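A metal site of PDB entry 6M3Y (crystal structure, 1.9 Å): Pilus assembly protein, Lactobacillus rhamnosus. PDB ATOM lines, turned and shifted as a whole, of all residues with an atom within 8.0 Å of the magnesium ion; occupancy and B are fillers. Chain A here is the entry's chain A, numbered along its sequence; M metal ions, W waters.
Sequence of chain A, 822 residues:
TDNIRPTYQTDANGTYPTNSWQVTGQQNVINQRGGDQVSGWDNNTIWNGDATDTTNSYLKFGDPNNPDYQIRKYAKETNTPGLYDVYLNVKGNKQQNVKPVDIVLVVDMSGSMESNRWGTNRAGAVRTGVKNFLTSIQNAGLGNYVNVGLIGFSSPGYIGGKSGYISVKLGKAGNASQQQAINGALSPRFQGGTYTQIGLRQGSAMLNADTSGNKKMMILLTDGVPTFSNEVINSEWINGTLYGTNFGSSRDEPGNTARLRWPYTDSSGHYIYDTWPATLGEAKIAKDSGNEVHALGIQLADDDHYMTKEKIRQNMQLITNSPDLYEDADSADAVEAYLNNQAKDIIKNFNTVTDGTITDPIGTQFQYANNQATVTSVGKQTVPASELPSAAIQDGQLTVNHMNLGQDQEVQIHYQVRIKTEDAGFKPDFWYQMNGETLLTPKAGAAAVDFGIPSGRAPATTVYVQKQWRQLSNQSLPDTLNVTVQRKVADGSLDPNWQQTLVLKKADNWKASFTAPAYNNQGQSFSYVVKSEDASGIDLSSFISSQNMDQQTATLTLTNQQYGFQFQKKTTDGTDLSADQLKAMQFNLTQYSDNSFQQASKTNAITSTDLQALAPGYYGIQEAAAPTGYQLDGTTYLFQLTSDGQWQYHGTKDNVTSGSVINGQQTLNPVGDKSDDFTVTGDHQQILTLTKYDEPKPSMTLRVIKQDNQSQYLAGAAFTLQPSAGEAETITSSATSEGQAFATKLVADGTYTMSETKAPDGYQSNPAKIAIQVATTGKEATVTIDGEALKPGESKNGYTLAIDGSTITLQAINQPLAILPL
The side-chain carboxylate of Asp 223 sits close to the side-chain hydroxyl of Ser 112 (2.5 Å). The guanidinium group (NH1) of Arg 122 lies within hydrogen-bond range of the backbone carbonyl oxygen (O) of Ser 112, 3.0 Å away. The backbone NH (N) of Ser 110 lies within hydrogen-bond range of the side-chain carboxylate (OD1) of Asp 108. The backbone carbonyl oxygen (O) of Thr 194 lies within hydrogen-bond range of the backbone NH (N) of Thr 227 (2.9 Å).
The magnesium ion is bound by water W2 (2.1 Å), water W1 (2.1 Å), the side-chain hydroxyl (OG) of Ser 112 (2.1 Å), the side-chain hydroxyl (OG) of Ser 110 (2.1 Å) and the side-chain hydroxyl (OG1) of Thr 194 (2.1 Å). The magnesium ion has five donor atoms within binding distance.
Water W2 lies within hydrogen-bond range of OD1 of Asp 223 and OD2 of Asp 108.
Of the 25 residues printed, 3 come within 4 Å of the magnesium ion. The nearest printed residue that does not touch the magnesium ion is Asp 223 (4.1 Å).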
ATOM      1  N   ASP A 108       9.773   5.228 -17.876  1.00  0.00           N
ATOM      2  CA  ASP A 108      11.227   5.245 -17.902  1.00  0.00           C
ATOM      3  C   ASP A 108      11.670   4.138 -18.848  1.00  0.00           C
ATOM      4  O   ASP A 108      11.577   2.960 -18.510  1.00  0.00           O
ATOM      5  CB  ASP A 108      11.707   4.967 -16.492  1.00  0.00           C
ATOM      6  CG  ASP A 108      13.188   4.923 -16.346  1.00  0.00           C
ATOM      7  OD1 ASP A 108      13.900   4.785 -17.370  1.00  0.00           O
ATOM      8  OD2 ASP A 108      13.638   5.046 -15.183  1.00  0.00           O
ATOM      9  N   MET A 109      12.122   4.527 -20.052  1.00  0.00           N
ATOM     10  CA  MET A 109      12.687   3.570 -21.005  1.00  0.00           C
ATOM     11  C   MET A 109      14.228   3.559 -21.013  1.00  0.00           C
ATOM     12  O   MET A 109      14.845   3.169 -21.997  1.00  0.00           O
ATOM     13  CB  MET A 109      12.105   3.811 -22.399  1.00  0.00           C
ATOM     14  CG  MET A 109      10.618   3.500 -22.394  1.00  0.00           C
ATOM     15  SD  MET A 109       9.764   3.954 -23.886  1.00  0.00           S
ATOM     16  CE  MET A 109      10.220   2.596 -24.952  1.00  0.00           C
ATOM     17  N   SER A 110      14.840   3.944 -19.884  1.00  0.00           N
ATOM     18  CA  SER A 110      16.301   3.944 -19.761  1.00  0.00           C
ATOM     19  C   SER A 110      16.881   2.542 -19.697  1.00  0.00           C
ATOM     20  O   SER A 110      16.157   1.553 -19.438  1.00  0.00           O
ATOM     21  CB  SER A 110      16.755   4.771 -18.545  1.00  0.00           C
ATOM     22  OG  SER A 110      16.481   4.104 -17.314  1.00  0.00           O
ATOM     23  N   GLY A 111      18.182   2.446 -19.967  1.00  0.00           N
ATOM     24  CA  GLY A 111      18.903   1.182 -20.026  1.00  0.00           C
ATOM     25  C   GLY A 111      18.904   0.456 -18.691  1.00  0.00           C
ATOM     26  O   GLY A 111      18.871  -0.770 -18.669  1.00  0.00           O
ATOM     27  N   SER A 112      18.906   1.229 -17.598  1.00  0.00           N
ATOM     28  CA  SER A 112      18.850   0.690 -16.244  1.00  0.00           C
ATOM     29  C   SER A 112      17.596  -0.112 -15.995  1.00  0.00           C
ATOM     30  O   SER A 112      17.548  -0.875 -15.050  1.00  0.00           O
ATOM     31  CB  SER A 112      19.006   1.796 -15.158  1.00  0.00           C
ATOM     32  OG  SER A 112      17.885   2.646 -15.070  1.00  0.00           O
ATOM     33  N   MET A 113      16.571   0.063 -16.840  1.00  0.00           N
ATOM     34  CA  MET A 113      15.325  -0.714 -16.772  1.00  0.00           C
ATOM     35  C   MET A 113      15.358  -2.058 -17.477  1.00  0.00           C
ATOM     36  O   MET A 113      14.403  -2.834 -17.363  1.00  0.00           O
ATOM     37  CB  MET A 113      14.166   0.096 -17.351  1.00  0.00           C
ATOM     38  CG  MET A 113      13.887   1.380 -16.578  1.00  0.00           C
ATOM     39  SD  MET A 113      12.853   1.116 -15.118  1.00  0.00           S
ATOM     40  CE  MET A 113      11.379   0.463 -15.896  1.00  0.00           C
ATOM     41  N   GLU A 114      16.445  -2.356 -18.198  1.00  0.00           N
ATOM     42  CA  GLU A 114      16.512  -3.625 -18.936  1.00  0.00           C
ATOM     43  C   GLU A 114      17.930  -4.019 -19.259  1.00  0.00           C
ATOM     44  O   GLU A 114      18.484  -3.445 -20.191  1.00  0.00           O
ATOM     45  CB  GLU A 114      15.680  -3.512 -20.236  1.00  0.00           C
ATOM     46  CG  GLU A 114      15.537  -4.816 -20.999  1.00  0.00           C
ATOM     47  CD  GLU A 114      14.563  -4.747 -22.176  1.00  0.00           C
ATOM     48  OE1 GLU A 114      14.053  -3.649 -22.510  1.00  0.00           O
ATOM     49  OE2 GLU A 114      14.297  -5.811 -22.787  1.00  0.00           O
ATOM     50  N   ARG A 122      13.023  -5.369 -15.249  1.00  0.00           N
ATOM     51  CA  ARG A 122      11.978  -4.385 -15.082  1.00  0.00           C
ATOM     52  C   ARG A 122      11.062  -4.219 -16.320  1.00  0.00           C
ATOM     53  O   ARG A 122       9.861  -4.444 -16.244  1.00  0.00           O
ATOM     54  CB  ARG A 122      12.593  -3.054 -14.687  1.00  0.00           C
ATOM     55  CG  ARG A 122      13.347  -3.106 -13.376  1.00  0.00           C
ATOM     56  CD  ARG A 122      13.771  -1.713 -12.949  1.00  0.00           C
ATOM     57  NE  ARG A 122      14.644  -1.692 -11.782  1.00  0.00           N
ATOM     58  CZ  ARG A 122      15.913  -2.092 -11.770  1.00  0.00           C
ATOM     59  NH1 ARG A 122      16.490  -2.589 -12.856  1.00  0.00           N
ATOM     60  NH2 ARG A 122      16.619  -2.008 -10.644  1.00  0.00           N
ATOM     61  N   PHE A 153      10.536   7.877 -21.992  1.00  0.00           N
ATOM     62  CA  PHE A 153      11.764   8.657 -22.061  1.00  0.00           C
ATOM     63  C   PHE A 153      13.028   7.847 -21.873  1.00  0.00           C
ATOM     64  O   PHE A 153      13.023   6.808 -21.182  1.00  0.00           O
ATOM     65  CB  PHE A 153      11.743   9.805 -21.079  1.00  0.00           C
ATOM     66  CG  PHE A 153      11.719   9.379 -19.653  1.00  0.00           C
ATOM     67  CD1 PHE A 153      12.895   9.182 -18.969  1.00  0.00           C
ATOM     68  CD2 PHE A 153      10.518   9.184 -18.982  1.00  0.00           C
ATOM     69  CE1 PHE A 153      12.888   8.806 -17.637  1.00  0.00           C
ATOM     70  CE2 PHE A 153      10.501   8.807 -17.666  1.00  0.00           C
ATOM     71  CZ  PHE A 153      11.687   8.629 -16.989  1.00  0.00           C
ATOM     72  N   SER A 154      14.101   8.331 -22.520  1.00  0.00           N
ATOM     73  CA  SER A 154      15.467   7.931 -22.262  1.00  0.00           C
ATOM     74  C   SER A 154      16.318   9.221 -22.161  1.00  0.00           C
ATOM     75  O   SER A 154      16.206   9.929 -21.172  1.00  0.00           O
ATOM     76  CB  SER A 154      15.986   6.952 -23.338  1.00  0.00           C
ATOM     77  OG  SER A 154      15.946   7.508 -24.646  1.00  0.00           O
ATOM     78  N   GLN A 191      16.692   1.447 -23.416  1.00  0.00           N
ATOM     79  CA  GLN A 191      18.116   1.777 -23.478  1.00  0.00           C
ATOM     80  C   GLN A 191      18.297   3.276 -23.361  1.00  0.00           C
ATOM     81  O   GLN A 191      17.409   4.067 -23.706  1.00  0.00           O
ATOM     82  CB  GLN A 191      18.798   1.265 -24.791  1.00  0.00           C
ATOM     83  CG  GLN A 191      17.985   1.558 -26.070  1.00  0.00           C
ATOM     84  CD  GLN A 191      18.811   1.838 -27.335  1.00  0.00           C
ATOM     85  OE1 GLN A 191      19.813   1.190 -27.600  1.00  0.00           O
ATOM     86  NE2 GLN A 191      18.344   2.812 -28.148  1.00  0.00           N
ATOM     87  N   GLY A 192      19.491   3.655 -22.910  1.00  0.00           N
ATOM     88  CA  GLY A 192      19.889   5.038 -22.805  1.00  0.00           C
ATOM     89  C   GLY A 192      19.803   5.582 -21.386  1.00  0.00           C
ATOM     90  O   GLY A 192      19.646   4.841 -20.435  1.00  0.00           O
ATOM     91  N   GLY A 193      19.930   6.910 -21.269  1.00  0.00           N
ATOM     92  CA  GLY A 193      19.905   7.589 -19.994  1.00  0.00           C
ATOM     93  C   GLY A 193      18.491   7.825 -19.495  1.00  0.00           C
ATOM     94  O   GLY A 193      17.528   7.401 -20.119  1.00  0.00           O
ATOM     95  N   THR A 194      18.400   8.526 -18.368  1.00  0.00           N
ATOM     96  CA  THR A 194      17.178   8.654 -17.597  1.00  0.00           C
ATOM     97  C   THR A 194      16.887  10.126 -17.381  1.00  0.00           C
ATOM     98  O   THR A 194      17.239  10.712 -16.368  1.00  0.00           O
ATOM     99  CB  THR A 194      17.276   7.890 -16.238  1.00  0.00           C
ATOM    100  OG1 THR A 194      17.792   6.586 -16.452  1.00  0.00           O
ATOM    101  CG2 THR A 194      15.907   7.761 -15.583  1.00  0.00           C
ATOM    102  N   TYR A 195      16.203  10.726 -18.359  1.00  0.00           N
ATOM    103  CA  TYR A 195      15.863  12.120 -18.358  1.00  0.00           C
ATOM    104  C   TYR A 195      14.429  12.263 -17.822  1.00  0.00           C
ATOM    105  O   TYR A 195      13.502  12.693 -18.521  1.00  0.00           O
ATOM    106  CB  TYR A 195      16.025  12.621 -19.787  1.00  0.00           C
ATOM    107  CG  TYR A 195      15.956  14.079 -20.056  1.00  0.00           C
ATOM    108  CD1 TYR A 195      15.941  15.028 -19.027  1.00  0.00           C
ATOM    109  CD2 TYR A 195      15.933  14.529 -21.373  1.00  0.00           C
ATOM    110  CE1 TYR A 195      15.903  16.382 -19.325  1.00  0.00           C
ATOM    111  CE2 TYR A 195      15.895  15.874 -21.681  1.00  0.00           C
ATOM    112  CZ  TYR A 195      15.880  16.787 -20.651  1.00  0.00           C
ATOM    113  OH  TYR A 195      15.828  18.091 -20.963  1.00  0.00           O
ATOM    114  N   THR A 196      14.264  11.932 -16.535  1.00  0.00           N
ATOM    115  CA  THR A 196      12.966  11.905 -15.890  1.00  0.00           C
ATOM    116  C   THR A 196      12.248  13.241 -15.987  1.00  0.00           C
ATOM    117  O   THR A 196      11.037  13.276 -16.202  1.00  0.00           O
ATOM    118  CB  THR A 196      13.114  11.502 -14.428  1.00  0.00           C
ATOM    119  OG1 THR A 196      13.936  10.337 -14.363  1.00  0.00           O
ATOM    120  CG2 THR A 196      11.751  11.239 -13.786  1.00  0.00           C
ATOM    121  N   THR A 222       9.311   4.109 -12.923  1.00  0.00           N
ATOM    122  CA  THR A 222      10.745   4.319 -12.999  1.00  0.00           C
ATOM    123  C   THR A 222      11.483   3.444 -11.989  1.00  0.00           C
ATOM    124  O   THR A 222      10.901   3.006 -11.009  1.00  0.00           O
ATOM    125  CB  THR A 222      11.056   5.808 -12.774  1.00  0.00           C
ATOM    126  OG1 THR A 222      12.421   6.045 -13.019  1.00  0.00           O
ATOM    127  CG2 THR A 222      10.747   6.220 -11.357  1.00  0.00           C
ATOM    128  N   ASP A 223      12.775   3.171 -12.238  1.00  0.00           N
ATOM    129  CA  ASP A 223      13.647   2.603 -11.188  1.00  0.00           C
ATOM    130  C   ASP A 223      14.297   3.674 -10.306  1.00  0.00           C
ATOM    131  O   ASP A 223      15.117   3.354  -9.427  1.00  0.00           O
ATOM    132  CB  ASP A 223      14.710   1.655 -11.752  1.00  0.00           C
ATOM    133  CG  ASP A 223      15.711   2.347 -12.628  1.00  0.00           C
ATOM    134  OD1 ASP A 223      16.014   3.534 -12.393  1.00  0.00           O
ATOM    135  OD2 ASP A 223      16.187   1.684 -13.580  1.00  0.00           O
ATOM    136  N   GLY A 224      13.965   4.951 -10.564  1.00  0.00           N
ATOM    137  CA  GLY A 224      14.162   6.024  -9.607  1.00  0.00           C
ATOM    138  C   GLY A 224      15.388   6.913  -9.689  1.00  0.00           C
ATOM    139  O   GLY A 224      15.456   7.887  -8.944  1.00  0.00           O
ATOM    140  N   VAL A 225      16.353   6.590 -10.545  1.00  0.00           N
ATOM    141  CA  VAL A 225      17.591   7.389 -10.621  1.00  0.00           C
ATOM    142  C   VAL A 225      17.683   8.238 -11.886  1.00  0.00           C
ATOM    143  O   VAL A 225      18.054   7.726 -12.941  1.00  0.00           O
ATOM    144  CB  VAL A 225      18.851   6.506 -10.546  1.00  0.00           C
ATOM    145  CG1 VAL A 225      20.061   7.396 -10.315  1.00  0.00           C
ATOM    146  CG2 VAL A 225      18.731   5.440  -9.470  1.00  0.00           C
ATOM    147  N   PRO A 226      17.359   9.559 -11.812  1.00  0.00           N
ATOM    148  CA  PRO A 226      17.493  10.427 -12.986  1.00  0.00           C
ATOM    149  C   PRO A 226      18.960  10.727 -13.259  1.00  0.00           C
ATOM    150  O   PRO A 226      19.640  11.157 -12.347  1.00  0.00           O
ATOM    151  CB  PRO A 226      16.741  11.713 -12.593  1.00  0.00           C
ATOM    152  CG  PRO A 226      16.229  11.497 -11.216  1.00  0.00           C
ATOM    153  CD  PRO A 226      16.885  10.283 -10.629  1.00  0.00           C
ATOM    154  N   THR A 227      19.420  10.458 -14.490  1.00  0.00           N
ATOM    155  CA  THR A 227      20.800  10.678 -14.885  1.00  0.00           C
ATOM    156  C   THR A 227      20.984  11.797 -15.907  1.00  0.00           C
ATOM    157  O   THR A 227      22.091  12.048 -16.348  1.00  0.00           O
ATOM    158  CB  THR A 227      21.427   9.391 -15.458  1.00  0.00           C
ATOM    159  OG1 THR A 227      20.777   9.014 -16.683  1.00  0.00           O
ATOM    160  CG2 THR A 227      21.354   8.264 -14.445  1.00  0.00           C
ATOM    161  N   GLY A 255      24.794  10.808 -16.600  1.00  0.00           N
ATOM    162  CA  GLY A 255      24.715   9.644 -17.474  1.00  0.00           C
ATOM    163  C   GLY A 255      24.333   8.335 -16.796  1.00  0.00           C
ATOM    164  O   GLY A 255      23.355   7.704 -17.196  1.00  0.00           O
ATOM    165  N   ASN A 256      25.096   7.938 -15.764  1.00  0.00           N
ATOM    166  CA  ASN A 256      24.865   6.663 -15.049  1.00  0.00           C
ATOM    167  C   ASN A 256      24.744   6.809 -13.506  1.00  0.00           C
ATOM    168  O   ASN A 256      24.872   5.839 -12.768  1.00  0.00           O
ATOM    169  CB  ASN A 256      25.936   5.624 -15.417  1.00  0.00           C
ATOM    170  CG  ASN A 256      27.319   5.977 -14.893  1.00  0.00           C
ATOM    171  OD1 ASN A 256      27.554   7.048 -14.322  1.00  0.00           O
ATOM    172  ND2 ASN A 256      28.260   5.078 -15.104  1.00  0.00           N
ATOM    173  N   THR A 257      24.511   8.035 -13.040  1.00  0.00           N
ATOM    174  CA  THR A 257      24.277   8.337 -11.632  1.00  0.00           C
ATOM    175  C   THR A 257      23.631   9.686 -11.643  1.00  0.00           C
ATOM    176  O   THR A 257      23.632  10.344 -12.674  1.00  0.00           O
ATOM    177  CB  THR A 257      25.595   8.373 -10.804  1.00  0.00           C
ATOM    178  OG1 THR A 257      25.302   8.779  -9.456  1.00  0.00           O
ATOM    179  CG2 THR A 257      26.623   9.342 -11.422  1.00  0.00           C
HETATM  180 MG    MG M   1      17.906   4.583 -15.860  1.00  0.00          MG
HETATM  181  O   HOH W   1      18.909   5.317 -14.179  1.00  0.00           O
HETATM  182  O   HOH W   2      16.190   4.695 -14.720  1.00  0.00           O
